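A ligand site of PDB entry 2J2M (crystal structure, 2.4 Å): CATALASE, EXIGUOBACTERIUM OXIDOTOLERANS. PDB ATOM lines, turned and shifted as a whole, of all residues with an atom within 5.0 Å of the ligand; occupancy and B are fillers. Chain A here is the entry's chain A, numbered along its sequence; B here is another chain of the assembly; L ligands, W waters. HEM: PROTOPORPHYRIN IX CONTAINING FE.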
ATOM      1  N   ARG A  53     -26.734   6.794  -3.240  1.00  0.00           N
ATOM      2  CA  ARG A  53     -26.663   7.388  -4.553  1.00  0.00           C
ATOM      3  C   ARG A  53     -26.200   8.833  -4.417  1.00  0.00           C
ATOM      4  O   ARG A  53     -26.626   9.549  -3.493  1.00  0.00           O
ATOM      5  CB  ARG A  53     -28.043   7.336  -5.230  1.00  0.00           C
ATOM      6  CG  ARG A  53     -28.422   5.973  -5.873  1.00  0.00           C
ATOM      7  CD  ARG A  53     -29.955   5.781  -5.914  1.00  0.00           C
ATOM      8  NE  ARG A  53     -30.424   4.484  -6.447  1.00  0.00           N
ATOM      9  CZ  ARG A  53     -30.352   3.345  -5.786  1.00  0.00           C
ATOM     10  NH1 ARG A  53     -29.824   3.311  -4.552  1.00  0.00           N
ATOM     11  NH2 ARG A  53     -30.767   2.243  -6.352  1.00  0.00           N
ATOM     12  N   VAL A  54     -25.336   9.281  -5.335  1.00  0.00           N
ATOM     13  CA  VAL A  54     -24.834  10.668  -5.290  1.00  0.00           C
ATOM     14  C   VAL A  54     -25.999  11.646  -5.299  1.00  0.00           C
ATOM     15  O   VAL A  54     -26.005  12.651  -4.529  1.00  0.00           O
ATOM     16  CB  VAL A  54     -23.772  10.952  -6.428  1.00  0.00           C
ATOM     17  CG1 VAL A  54     -24.320  10.636  -7.775  1.00  0.00           C
ATOM     18  CG2 VAL A  54     -23.309  12.400  -6.419  1.00  0.00           C
ATOM     19  N   VAL A  55     -26.996  11.362  -6.149  1.00  0.00           N
ATOM     20  CA  VAL A  55     -28.299  12.069  -6.097  1.00  0.00           C
ATOM     21  C   VAL A  55     -29.369  10.996  -6.153  1.00  0.00           C
ATOM     22  O   VAL A  55     -29.102   9.856  -6.524  1.00  0.00           O
ATOM     23  CB  VAL A  55     -28.505  13.127  -7.224  1.00  0.00           C
ATOM     24  CG1 VAL A  55     -27.626  14.350  -7.005  1.00  0.00           C
ATOM     25  CG2 VAL A  55     -28.315  12.530  -8.642  1.00  0.00           C
ATOM     26  N   HIS A  56     -30.587  11.355  -5.763  1.00  0.00           N
ATOM     27  CA  HIS A  56     -31.716  10.436  -5.770  1.00  0.00           C
ATOM     28  C   HIS A  56     -31.546   9.294  -4.793  1.00  0.00           C
ATOM     29  O   HIS A  56     -32.010   8.183  -5.064  1.00  0.00           O
ATOM     30  CB  HIS A  56     -31.963   9.827  -7.155  1.00  0.00           C
ATOM     31  CG  HIS A  56     -32.472  10.800  -8.174  1.00  0.00           C
ATOM     32  ND1 HIS A  56     -33.808  10.891  -8.520  1.00  0.00           N
ATOM     33  CD2 HIS A  56     -31.812  11.673  -8.978  1.00  0.00           C
ATOM     34  CE1 HIS A  56     -33.953  11.794  -9.474  1.00  0.00           C
ATOM     35  NE2 HIS A  56     -32.757  12.272  -9.788  1.00  0.00           N
ATOM     36  N   ARG A  93     -38.067   2.117  -9.734  1.00  0.00           N
ATOM     37  CA  ARG A  93     -37.610   2.868  -8.558  1.00  0.00           C
ATOM     38  C   ARG A  93     -37.977   4.330  -8.744  1.00  0.00           C
ATOM     39  O   ARG A  93     -37.639   4.930  -9.761  1.00  0.00           O
ATOM     40  CB  ARG A  93     -36.082   2.719  -8.296  1.00  0.00           C
ATOM     41  CG  ARG A  93     -35.589   3.475  -7.038  1.00  0.00           C
ATOM     42  CD  ARG A  93     -34.153   3.135  -6.622  1.00  0.00           C
ATOM     43  NE  ARG A  93     -33.719   3.701  -5.318  1.00  0.00           N
ATOM     44  CZ  ARG A  93     -33.328   4.978  -5.109  1.00  0.00           C
ATOM     45  NH1 ARG A  93     -33.363   5.871  -6.114  1.00  0.00           N
ATOM     46  NH2 ARG A  93     -32.927   5.363  -3.896  1.00  0.00           N
ATOM     47  N   SER A  95     -38.033   8.198  -6.671  1.00  0.00           N
ATOM     48  CA  SER A  95     -37.035   8.818  -5.796  1.00  0.00           C
ATOM     49  C   SER A  95     -37.210  10.309  -5.722  1.00  0.00           C
ATOM     50  O   SER A  95     -37.909  10.886  -6.560  1.00  0.00           O
ATOM     51  CB  SER A  95     -35.610   8.472  -6.273  1.00  0.00           C
ATOM     52  OG  SER A  95     -35.392   8.893  -7.605  1.00  0.00           O
ATOM     53  N   GLY A 112     -37.644  11.283  -9.360  1.00  0.00           N
ATOM     54  CA  GLY A 112     -37.103  10.260 -10.244  1.00  0.00           C
ATOM     55  C   GLY A 112     -38.119   9.172 -10.577  1.00  0.00           C
ATOM     56  O   GLY A 112     -38.920   8.763  -9.712  1.00  0.00           O
ATOM     57  N   PHE A 113     -38.068   8.700 -11.821  1.00  0.00           N
ATOM     58  CA  PHE A 113     -38.964   7.696 -12.386  1.00  0.00           C
ATOM     59  C   PHE A 113     -38.137   6.697 -13.235  1.00  0.00           C
ATOM     60  O   PHE A 113     -37.870   6.919 -14.423  1.00  0.00           O
ATOM     61  CB  PHE A 113     -40.052   8.411 -13.235  1.00  0.00           C
ATOM     62  CG  PHE A 113     -41.232   7.540 -13.626  1.00  0.00           C
ATOM     63  CD1 PHE A 113     -41.042   6.320 -14.260  1.00  0.00           C
ATOM     64  CD2 PHE A 113     -42.534   7.978 -13.383  1.00  0.00           C
ATOM     65  CE1 PHE A 113     -42.136   5.533 -14.626  1.00  0.00           C
ATOM     66  CE2 PHE A 113     -43.635   7.218 -13.745  1.00  0.00           C
ATOM     67  CZ  PHE A 113     -43.426   5.989 -14.376  1.00  0.00           C
ATOM     68  N   SER A 114     -37.704   5.611 -12.610  1.00  0.00           N
ATOM     69  CA  SER A 114     -36.776   4.682 -13.248  1.00  0.00           C
ATOM     70  C   SER A 114     -37.420   3.293 -13.432  1.00  0.00           C
ATOM     71  O   SER A 114     -38.002   2.730 -12.494  1.00  0.00           O
ATOM     72  CB  SER A 114     -35.469   4.555 -12.423  1.00  0.00           C
ATOM     73  OG  SER A 114     -34.778   5.792 -12.327  1.00  0.00           O
ATOM     74  N   VAL A 127     -34.862   5.974 -17.493  1.00  0.00           N
ATOM     75  CA  VAL A 127     -34.429   6.739 -16.308  1.00  0.00           C
ATOM     76  C   VAL A 127     -34.832   8.191 -16.535  1.00  0.00           C
ATOM     77  O   VAL A 127     -34.118   8.955 -17.193  1.00  0.00           O
ATOM     78  CB  VAL A 127     -32.891   6.563 -16.040  1.00  0.00           C
ATOM     79  CG1 VAL A 127     -32.448   7.280 -14.755  1.00  0.00           C
ATOM     80  CG2 VAL A 127     -32.539   5.068 -15.968  1.00  0.00           C
ATOM     81  N   GLY A 128     -36.014   8.555 -16.062  1.00  0.00           N
ATOM     82  CA  GLY A 128     -36.550   9.892 -16.234  1.00  0.00           C
ATOM     83  C   GLY A 128     -36.944  10.539 -14.909  1.00  0.00           C
ATOM     84  O   GLY A 128     -36.660  10.002 -13.842  1.00  0.00           O
ATOM     85  N   ASN A 129     -37.584  11.714 -15.007  1.00  0.00           N
ATOM     86  CA  ASN A 129     -38.165  12.452 -13.887  1.00  0.00           C
ATOM     87  C   ASN A 129     -39.647  12.706 -14.193  1.00  0.00           C
ATOM     88  O   ASN A 129     -40.085  12.545 -15.340  1.00  0.00           O
ATOM     89  CB  ASN A 129     -37.442  13.788 -13.702  1.00  0.00           C
ATOM     90  CG  ASN A 129     -36.153  13.680 -12.891  1.00  0.00           C
ATOM     91  OD1 ASN A 129     -35.967  12.739 -12.115  1.00  0.00           O
ATOM     92  ND2 ASN A 129     -35.263  14.669 -13.038  1.00  0.00           N
ATOM     93  N   PHE A 134     -35.332  19.923 -17.867  1.00  0.00           N
ATOM     94  CA  PHE A 134     -34.259  20.039 -16.882  1.00  0.00           C
ATOM     95  C   PHE A 134     -33.705  21.461 -16.727  1.00  0.00           C
ATOM     96  O   PHE A 134     -33.984  22.351 -17.567  1.00  0.00           O
ATOM     97  CB  PHE A 134     -33.122  19.033 -17.152  1.00  0.00           C
ATOM     98  CG  PHE A 134     -32.501  18.491 -15.911  1.00  0.00           C
ATOM     99  CD1 PHE A 134     -31.185  18.770 -15.616  1.00  0.00           C
ATOM    100  CD2 PHE A 134     -33.255  17.742 -15.003  1.00  0.00           C
ATOM    101  CE1 PHE A 134     -30.571  18.258 -14.435  1.00  0.00           C
ATOM    102  CE2 PHE A 134     -32.693  17.246 -13.824  1.00  0.00           C
ATOM    103  CZ  PHE A 134     -31.320  17.491 -13.552  1.00  0.00           C
ATOM    104  N   ALA A 139     -23.878  18.223 -19.647  1.00  0.00           N
ATOM    105  CA  ALA A 139     -23.457  17.443 -18.492  1.00  0.00           C
ATOM    106  C   ALA A 139     -22.333  18.139 -17.725  1.00  0.00           C
ATOM    107  O   ALA A 139     -22.167  17.915 -16.526  1.00  0.00           O
ATOM    108  CB  ALA A 139     -23.014  16.071 -18.938  1.00  0.00           C
ATOM    109  N   PHE A 142     -23.524  19.737 -14.497  1.00  0.00           N
ATOM    110  CA  PHE A 142     -24.337  18.946 -13.548  1.00  0.00           C
ATOM    111  C   PHE A 142     -23.764  18.918 -12.118  1.00  0.00           C
ATOM    112  O   PHE A 142     -24.500  19.130 -11.155  1.00  0.00           O
ATOM    113  CB  PHE A 142     -24.612  17.521 -14.084  1.00  0.00           C
ATOM    114  CG  PHE A 142     -25.569  16.736 -13.231  1.00  0.00           C
ATOM    115  CD1 PHE A 142     -26.941  17.022 -13.246  1.00  0.00           C
ATOM    116  CD2 PHE A 142     -25.113  15.719 -12.375  1.00  0.00           C
ATOM    117  CE1 PHE A 142     -27.842  16.302 -12.443  1.00  0.00           C
ATOM    118  CE2 PHE A 142     -26.005  15.003 -11.586  1.00  0.00           C
ATOM    119  CZ  PHE A 142     -27.371  15.307 -11.613  1.00  0.00           C
ATOM    120  N   SER A 197     -39.140  11.137 -20.261  1.00  0.00           N
ATOM    121  CA  SER A 197     -37.746  10.845 -20.649  1.00  0.00           C
ATOM    122  C   SER A 197     -36.903  12.104 -20.544  1.00  0.00           C
ATOM    123  O   SER A 197     -35.682  12.041 -20.346  1.00  0.00           O
ATOM    124  CB  SER A 197     -37.661  10.271 -22.059  1.00  0.00           C
ATOM    125  OG  SER A 197     -38.294  11.120 -22.985  1.00  0.00           O
ATOM    126  N   VAL A 198     -37.580  13.251 -20.661  1.00  0.00           N
ATOM    127  CA  VAL A 198     -36.951  14.575 -20.730  1.00  0.00           C
ATOM    128  C   VAL A 198     -36.125  14.778 -22.029  1.00  0.00           C
ATOM    129  O   VAL A 198     -36.374  15.748 -22.760  1.00  0.00           O
ATOM    130  CB  VAL A 198     -36.153  14.923 -19.420  1.00  0.00           C
ATOM    131  CG1 VAL A 198     -35.362  16.249 -19.581  1.00  0.00           C
ATOM    132  CG2 VAL A 198     -37.117  14.972 -18.230  1.00  0.00           C
ATOM    133  N   HIS A 199     -35.150  13.896 -22.276  1.00  0.00           N
ATOM    134  CA  HIS A 199     -34.389  13.877 -23.529  1.00  0.00           C
ATOM    135  C   HIS A 199     -35.143  13.200 -24.666  1.00  0.00           C
ATOM    136  O   HIS A 199     -36.017  12.365 -24.433  1.00  0.00           O
ATOM    137  CB  HIS A 199     -33.075  13.106 -23.364  1.00  0.00           C
ATOM    138  CG  HIS A 199     -32.353  13.378 -22.072  1.00  0.00           C
ATOM    139  ND1 HIS A 199     -31.717  14.578 -21.807  1.00  0.00           N
ATOM    140  CD2 HIS A 199     -32.145  12.599 -20.987  1.00  0.00           C
ATOM    141  CE1 HIS A 199     -31.159  14.521 -20.618  1.00  0.00           C
ATOM    142  NE2 HIS A 199     -31.408  13.327 -20.097  1.00  0.00           N
ATOM    143  N   VAL A 313     -30.031  -1.953  -7.079  1.00  0.00           N
ATOM    144  CA  VAL A 313     -30.248  -1.712  -8.493  1.00  0.00           C
ATOM    145  C   VAL A 313     -29.448  -0.504  -9.014  1.00  0.00           C
ATOM    146  O   VAL A 313     -29.290   0.493  -8.315  1.00  0.00           O
ATOM    147  CB  VAL A 313     -31.771  -1.561  -8.874  1.00  0.00           C
ATOM    148  CG1 VAL A 313     -32.396  -0.248  -8.332  1.00  0.00           C
ATOM    149  CG2 VAL A 313     -31.992  -1.726 -10.400  1.00  0.00           C
ATOM    150  N   GLY A 314     -28.945  -0.630 -10.229  1.00  0.00           N
ATOM    151  CA  GLY A 314     -28.451   0.515 -10.960  1.00  0.00           C
ATOM    152  C   GLY A 314     -29.117   0.640 -12.309  1.00  0.00           C
ATOM    153  O   GLY A 314     -29.321  -0.355 -13.001  1.00  0.00           O
ATOM    154  N   PHE A 315     -29.477   1.873 -12.689  1.00  0.00           N
ATOM    155  CA  PHE A 315     -30.022   2.143 -14.012  1.00  0.00           C
ATOM    156  C   PHE A 315     -29.153   3.138 -14.781  1.00  0.00           C
ATOM    157  O   PHE A 315     -28.422   3.927 -14.185  1.00  0.00           O
ATOM    158  CB  PHE A 315     -31.418   2.766 -13.940  1.00  0.00           C
ATOM    159  CG  PHE A 315     -32.382   2.099 -13.005  1.00  0.00           C
ATOM    160  CD1 PHE A 315     -33.311   1.181 -13.502  1.00  0.00           C
ATOM    161  CD2 PHE A 315     -32.448   2.481 -11.663  1.00  0.00           C
ATOM    162  CE1 PHE A 315     -34.264   0.623 -12.640  1.00  0.00           C
ATOM    163  CE2 PHE A 315     -33.384   1.922 -10.819  1.00  0.00           C
ATOM    164  CZ  PHE A 315     -34.295   0.985 -11.302  1.00  0.00           C
ATOM    165  N   LEU A 331     -26.854  17.034 -22.462  1.00  0.00           N
ATOM    166  CA  LEU A 331     -27.029  16.619 -21.092  1.00  0.00           C
ATOM    167  C   LEU A 331     -27.077  15.061 -21.034  1.00  0.00           C
ATOM    168  O   LEU A 331     -26.373  14.440 -20.243  1.00  0.00           O
ATOM    169  CB  LEU A 331     -28.281  17.267 -20.507  1.00  0.00           C
ATOM    170  CG  LEU A 331     -28.502  17.138 -19.001  1.00  0.00           C
ATOM    171  CD1 LEU A 331     -27.561  18.040 -18.200  1.00  0.00           C
ATOM    172  CD2 LEU A 331     -29.984  17.401 -18.667  1.00  0.00           C
ATOM    173  N   GLY A 334     -23.600  12.915 -21.224  1.00  0.00           N
ATOM    174  CA  GLY A 334     -22.797  12.728 -20.024  1.00  0.00           C
ATOM    175  C   GLY A 334     -23.368  11.651 -19.124  1.00  0.00           C
ATOM    176  O   GLY A 334     -22.633  10.884 -18.499  1.00  0.00           O
ATOM    177  N   ARG A 335     -24.688  11.592 -19.044  1.00  0.00           N
ATOM    178  CA  ARG A 335     -25.365  10.534 -18.317  1.00  0.00           C
ATOM    179  C   ARG A 335     -24.953   9.137 -18.806  1.00  0.00           C
ATOM    180  O   ARG A 335     -24.715   8.232 -17.983  1.00  0.00           O
ATOM    181  CB  ARG A 335     -26.889  10.713 -18.366  1.00  0.00           C
ATOM    182  CG  ARG A 335     -27.410  11.963 -17.651  1.00  0.00           C
ATOM    183  CD  ARG A 335     -28.919  12.118 -17.877  1.00  0.00           C
ATOM    184  NE  ARG A 335     -29.754  11.271 -16.997  1.00  0.00           N
ATOM    185  CZ  ARG A 335     -30.959  10.799 -17.341  1.00  0.00           C
ATOM    186  NH1 ARG A 335     -31.454  11.060 -18.555  1.00  0.00           N
ATOM    187  NH2 ARG A 335     -31.654  10.066 -16.497  1.00  0.00           N
ATOM    188  N   SER A 338     -21.959   8.471 -16.813  1.00  0.00           N
ATOM    189  CA  SER A 338     -21.997   8.750 -15.369  1.00  0.00           C
ATOM    190  C   SER A 338     -22.598   7.644 -14.532  1.00  0.00           C
ATOM    191  O   SER A 338     -22.023   7.276 -13.512  1.00  0.00           O
ATOM    192  CB  SER A 338     -22.776  10.042 -15.122  1.00  0.00           C
ATOM    193  OG  SER A 338     -22.801  10.407 -13.743  1.00  0.00           O
ATOM    194  N   TYR A 339     -23.735   7.108 -14.979  1.00  0.00           N
ATOM    195  CA  TYR A 339     -24.520   6.135 -14.219  1.00  0.00           C
ATOM    196  C   TYR A 339     -23.769   4.851 -13.921  1.00  0.00           C
ATOM    197  O   TYR A 339     -23.587   4.488 -12.755  1.00  0.00           O
ATOM    198  CB  TYR A 339     -25.880   5.854 -14.902  1.00  0.00           C
ATOM    199  CG  TYR A 339     -26.873   6.990 -14.775  1.00  0.00           C
ATOM    200  CD1 TYR A 339     -27.943   6.922 -13.893  1.00  0.00           C
ATOM    201  CD2 TYR A 339     -26.708   8.172 -15.522  1.00  0.00           C
ATOM    202  CE1 TYR A 339     -28.876   7.998 -13.802  1.00  0.00           C
ATOM    203  CE2 TYR A 339     -27.557   9.202 -15.432  1.00  0.00           C
ATOM    204  CZ  TYR A 339     -28.650   9.145 -14.562  1.00  0.00           C
ATOM    205  OH  TYR A 339     -29.477  10.238 -14.509  1.00  0.00           O
ATOM    206  N   THR A 342     -20.562   5.518 -11.822  1.00  0.00           N
ATOM    207  CA  THR A 342     -20.817   5.662 -10.378  1.00  0.00           C
ATOM    208  C   THR A 342     -21.233   4.335  -9.737  1.00  0.00           C
ATOM    209  O   THR A 342     -20.966   4.120  -8.575  1.00  0.00           O
ATOM    210  CB  THR A 342     -21.894   6.718 -10.096  1.00  0.00           C
ATOM    211  OG1 THR A 342     -21.814   7.131  -8.710  1.00  0.00           O
ATOM    212  CG2 THR A 342     -23.322   6.205 -10.444  1.00  0.00           C
ATOM    213  N   GLN A 343     -21.900   3.475 -10.498  1.00  0.00           N
ATOM    214  CA  GLN A 343     -22.330   2.167 -10.011  1.00  0.00           C
ATOM    215  C   GLN A 343     -21.140   1.218  -9.797  1.00  0.00           C
ATOM    216  O   GLN A 343     -21.165   0.388  -8.885  1.00  0.00           O
ATOM    217  CB  GLN A 343     -23.381   1.569 -10.929  1.00  0.00           C
ATOM    218  CG  GLN A 343     -24.737   2.277 -10.825  1.00  0.00           C
ATOM    219  CD  GLN A 343     -25.518   2.309 -12.136  1.00  0.00           C
ATOM    220  OE1 GLN A 343     -25.284   1.496 -13.025  1.00  0.00           O
ATOM    221  NE2 GLN A 343     -26.457   3.229 -12.262  1.00  0.00           N
ATOM    222  N   ARG A 346     -20.227   2.633  -6.383  1.00  0.00           N
ATOM    223  CA  ARG A 346     -21.283   2.449  -5.383  1.00  0.00           C
ATOM    224  C   ARG A 346     -21.695   0.983  -5.112  1.00  0.00           C
ATOM    225  O   ARG A 346     -21.964   0.605  -3.973  1.00  0.00           O
ATOM    226  CB  ARG A 346     -22.517   3.305  -5.755  1.00  0.00           C
ATOM    227  CG  ARG A 346     -23.754   3.001  -4.906  1.00  0.00           C
ATOM    228  CD  ARG A 346     -24.929   3.959  -5.157  1.00  0.00           C
ATOM    229  NE  ARG A 346     -25.679   3.665  -6.397  1.00  0.00           N
ATOM    230  CZ  ARG A 346     -26.614   2.716  -6.519  1.00  0.00           C
ATOM    231  NH1 ARG A 346     -27.249   2.557  -7.668  1.00  0.00           N
ATOM    232  NH2 ARG A 346     -26.898   1.912  -5.521  1.00  0.00           N
ATOM    233  N   ILE B  42     -16.981  14.703 -13.915  1.00  0.00           N
ATOM    234  CA  ILE B  42     -18.106  13.801 -13.655  1.00  0.00           C
ATOM    235  C   ILE B  42     -17.670  12.590 -12.865  1.00  0.00           C
ATOM    236  O   ILE B  42     -18.382  12.112 -11.983  1.00  0.00           O
ATOM    237  CB  ILE B  42     -18.792  13.322 -14.980  1.00  0.00           C
ATOM    238  CG1 ILE B  42     -19.451  14.486 -15.733  1.00  0.00           C
ATOM    239  CG2 ILE B  42     -19.774  12.138 -14.711  1.00  0.00           C
ATOM    240  CD1 ILE B  42     -20.632  15.108 -14.993  1.00  0.00           C
ATOM    241  N   PHE B  45     -17.261  13.476  -9.212  1.00  0.00           N
ATOM    242  CA  PHE B  45     -18.639  13.645  -8.750  1.00  0.00           C
ATOM    243  C   PHE B  45     -19.308  12.311  -8.518  1.00  0.00           C
ATOM    244  O   PHE B  45     -20.054  12.170  -7.577  1.00  0.00           O
ATOM    245  CB  PHE B  45     -19.420  14.432  -9.773  1.00  0.00           C
ATOM    246  CG  PHE B  45     -20.873  14.511  -9.490  1.00  0.00           C
ATOM    247  CD1 PHE B  45     -21.366  15.414  -8.554  1.00  0.00           C
ATOM    248  CD2 PHE B  45     -21.779  13.698 -10.182  1.00  0.00           C
ATOM    249  CE1 PHE B  45     -22.732  15.501  -8.282  1.00  0.00           C
ATOM    250  CE2 PHE B  45     -23.127  13.785  -9.926  1.00  0.00           C
ATOM    251  CZ  PHE B  45     -23.609  14.696  -8.974  1.00  0.00           C
ATOM    252  N   ASP B  46     -19.006  11.337  -9.396  1.00  0.00           N
ATOM    253  CA  ASP B  46     -19.600   9.984  -9.320  1.00  0.00           C
ATOM    254  C   ASP B  46     -19.130   9.236  -8.085  1.00  0.00           C
ATOM    255  O   ASP B  46     -19.722   8.248  -7.717  1.00  0.00           O
ATOM    256  CB  ASP B  46     -19.253   9.155 -10.582  1.00  0.00           C
ATOM    257  CG  ASP B  46     -19.995   9.631 -11.845  1.00  0.00           C
ATOM    258  OD1 ASP B  46     -19.587   9.213 -12.984  1.00  0.00           O
ATOM    259  OD2 ASP B  46     -20.957  10.430 -11.723  1.00  0.00           O
HETATM  260  CHA HEM L   1     -29.472   9.305 -10.465  1.00  0.00           C
HETATM  261  CHB HEM L   1     -32.832  11.396 -13.328  1.00  0.00           C
HETATM  262  CHC HEM L   1     -29.423  14.281 -15.135  1.00  0.00           C
HETATM  263  CHD HEM L   1     -25.996  11.782 -12.825  1.00  0.00           C
HETATM  264  C1A HEM L   1     -30.680   9.579 -11.106  1.00  0.00           C
HETATM  265  C2A HEM L   1     -31.953   8.893 -10.922  1.00  0.00           C
HETATM  266  C3A HEM L   1     -32.879   9.472 -11.718  1.00  0.00           C
HETATM  267  C4A HEM L   1     -32.231  10.550 -12.423  1.00  0.00           C
HETATM  268  CMA HEM L   1     -34.376   9.102 -11.896  1.00  0.00           C
HETATM  269  CAA HEM L   1     -32.162   7.700  -9.957  1.00  0.00           C
HETATM  270  CBA HEM L   1     -31.970   6.338 -10.619  1.00  0.00           C
HETATM  271  CGA HEM L   1     -32.271   5.301  -9.560  1.00  0.00           C
HETATM  272  O1A HEM L   1     -31.338   4.571  -9.114  1.00  0.00           O
HETATM  273  O2A HEM L   1     -33.451   5.209  -9.139  1.00  0.00           O
HETATM  274  C1B HEM L   1     -32.204  12.311 -14.118  1.00  0.00           C
HETATM  275  C2B HEM L   1     -32.769  13.021 -15.256  1.00  0.00           C
HETATM  276  C3B HEM L   1     -31.812  13.808 -15.735  1.00  0.00           C
HETATM  277  C4B HEM L   1     -30.624  13.639 -14.933  1.00  0.00           C
HETATM  278  CMB HEM L   1     -34.199  12.849 -15.845  1.00  0.00           C
HETATM  279  CAB HEM L   1     -31.879  14.730 -16.962  1.00  0.00           C
HETATM  280  CBB HEM L   1     -32.951  15.472 -17.217  1.00  0.00           C
HETATM  281  C1C HEM L   1     -28.183  13.823 -14.759  1.00  0.00           C
HETATM  282  C2C HEM L   1     -26.894  14.252 -15.290  1.00  0.00           C
HETATM  283  C3C HEM L   1     -25.958  13.531 -14.632  1.00  0.00           C
HETATM  284  C4C HEM L   1     -26.627  12.651 -13.686  1.00  0.00           C
HETATM  285  CMC HEM L   1     -26.658  15.303 -16.410  1.00  0.00           C
HETATM  286  CAC HEM L   1     -24.423  13.611 -14.789  1.00  0.00           C
HETATM  287  CBC HEM L   1     -23.800  13.058 -15.832  1.00  0.00           C
HETATM  288  C1D HEM L   1     -26.579  10.903 -11.944  1.00  0.00           C
HETATM  289  C2D HEM L   1     -25.856  10.023 -11.053  1.00  0.00           C
HETATM  290  C3D HEM L   1     -26.941   9.229 -10.324  1.00  0.00           C
HETATM  291  C4D HEM L   1     -28.210   9.728 -10.837  1.00  0.00           C
HETATM  292  CMD HEM L   1     -24.296   9.871 -10.921  1.00  0.00           C
HETATM  293  CAD HEM L   1     -26.740   8.142  -9.260  1.00  0.00           C
HETATM  294  CBD HEM L   1     -27.006   6.792  -9.945  1.00  0.00           C
HETATM  295  CGD HEM L   1     -26.538   5.618  -9.101  1.00  0.00           C
HETATM  296  O1D HEM L   1     -25.810   5.779  -8.061  1.00  0.00           O
HETATM  297  O2D HEM L   1     -26.883   4.481  -9.502  1.00  0.00           O
HETATM  298  NA  HEM L   1     -30.902  10.584 -12.037  1.00  0.00           N
HETATM  299  NB  HEM L   1     -30.898  12.714 -13.943  1.00  0.00           N
HETATM  300  NC  HEM L   1     -27.969  12.849 -13.801  1.00  0.00           N
HETATM  301  ND  HEM L   1     -27.937  10.692 -11.793  1.00  0.00           N
HETATM  302 FE   HEM L   1     -29.375  11.491 -13.095  1.00  0.00          FE
HETATM  303  O   HOH W   1     -29.330   3.810 -10.698  1.00  0.00           O
HETATM  304  O   HOH W   2     -35.625   6.915  -9.566  1.00  0.00           O
HETATM  305  O   HOH W   3     -23.902   7.308  -7.036  1.00  0.00           O
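NE of Arg 53 lies within salt-bridge range of O1A of the ligand, 2.8 Å away. NE2 of Gln 343 sits at hydrogen-bond distance from O2D of the ligand, at 3.1 Å. NH1 of Arg 346 is in salt-bridge range of O2D of the ligand (2.7 Å). O2A of the ligand lies within salt-bridge range of NH1 of Arg 93 (3.1 Å). An iron atom (FE) of the ligand is bound by the side-chain hydroxyl (OH) of Tyr 339 (1.9 Å).
OG1 of Thr 342 lies within hydrogen-bond range of O of Asp 46 of chain B. O of Gly 128 sits at hydrogen-bond distance from N of Phe 113 (2.8 Å). The guanidinium group (NH1) of Arg 93 is in hydrogen-bond range of the backbone carbonyl oxygen (O) of His 56 (2.9 Å). The guanidinium group of Arg 346 lies within hydrogen-bond range of the backbone carbonyl oxygen of Val 313 (3.0 Å). The side-chain hydroxyl (OG) of Ser 197 lies within hydrogen-bond range of the backbone carbonyl oxygen (O) of His 199. The guanidinium group of Arg 53 lies within hydrogen-bond range of the backbone carbonyl oxygen of Val 313 (3.0 Å). NE2 of Gln 343 is in hydrogen-bond range of O of Phe 315, 2.8 Å away. The backbone carbonyl oxygen of Ser 114 sits at hydrogen-bond distance from the backbone NH of Arg 93 (2.8 Å).
A ring nitrogen (NE2) of His 56 sits close to a nitrogen (NA) of the ligand (3.4 Å). Merely in contact with the ligand: Val 54 (3.2 Å), Val 55 (3.6 Å), Gly 112 (3.4 Å), Phe 113 (3.7 Å), Ser 114 (3.3 Å), Val 127 (3.8 Å), Gly 128 (3.1 Å), Asn 129 (3.5 Å), Phe 134 (3.2 Å), Phe 142 (3.2 Å), Val 198 (3.5 Å), His 199 (3.5 Å), Phe 315 (3.5 Å), Leu 331 (3.4 Å), Gly 334 (3.6 Å), Arg 335 (3.3 Å), Ser 338 (3.2 Å), Thr 342 (3.5 Å), Ile 42 of chain B (3.9 Å) and Asp 46 of chain B (3.5 Å). Hydrophobic or aromatic side chains that line the ligand: Val 54, Val 55, His 56, Val 127, Phe 134, Phe 142, Val 198, His 199, Phe 315, Leu 331, Tyr 339 and Ile 42 of chain B. Within 4 Å of the ligand: Arg 53, Val 54, Val 55, His 56, Arg 93, Gly 112, Phe 113, Ser 114, Val 127, Gly 128, Asn 129, Phe 134, Phe 142, Val 198, His 199, Phe 315, Leu 331, Gly 334, Arg 335, Ser 338, Tyr 339, Thr 342, Gln 343, Arg 346, Ile 42 of chain B and Asp 46 of chain B. The nearest printed residue that does not touch the ligand is Ser 95 (4.2 Å).
Water W3 lies within hydrogen-bond range of O1D of the ligand (2.7 Å), OG1 of Thr 342 (2.7 Å) and N of Val 54 (3.0 Å). Water W1 lies within hydrogen-bond range of O1A of the ligand, N of Phe 315 and NE2 of Gln 343. Water W2 lies within hydrogen-bond range of OG of Ser 95 (2.8 Å), O2A of the ligand (2.8 Å), O of Arg 93 (2.8 Å) and OG of Ser 114 (3.1 Å).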
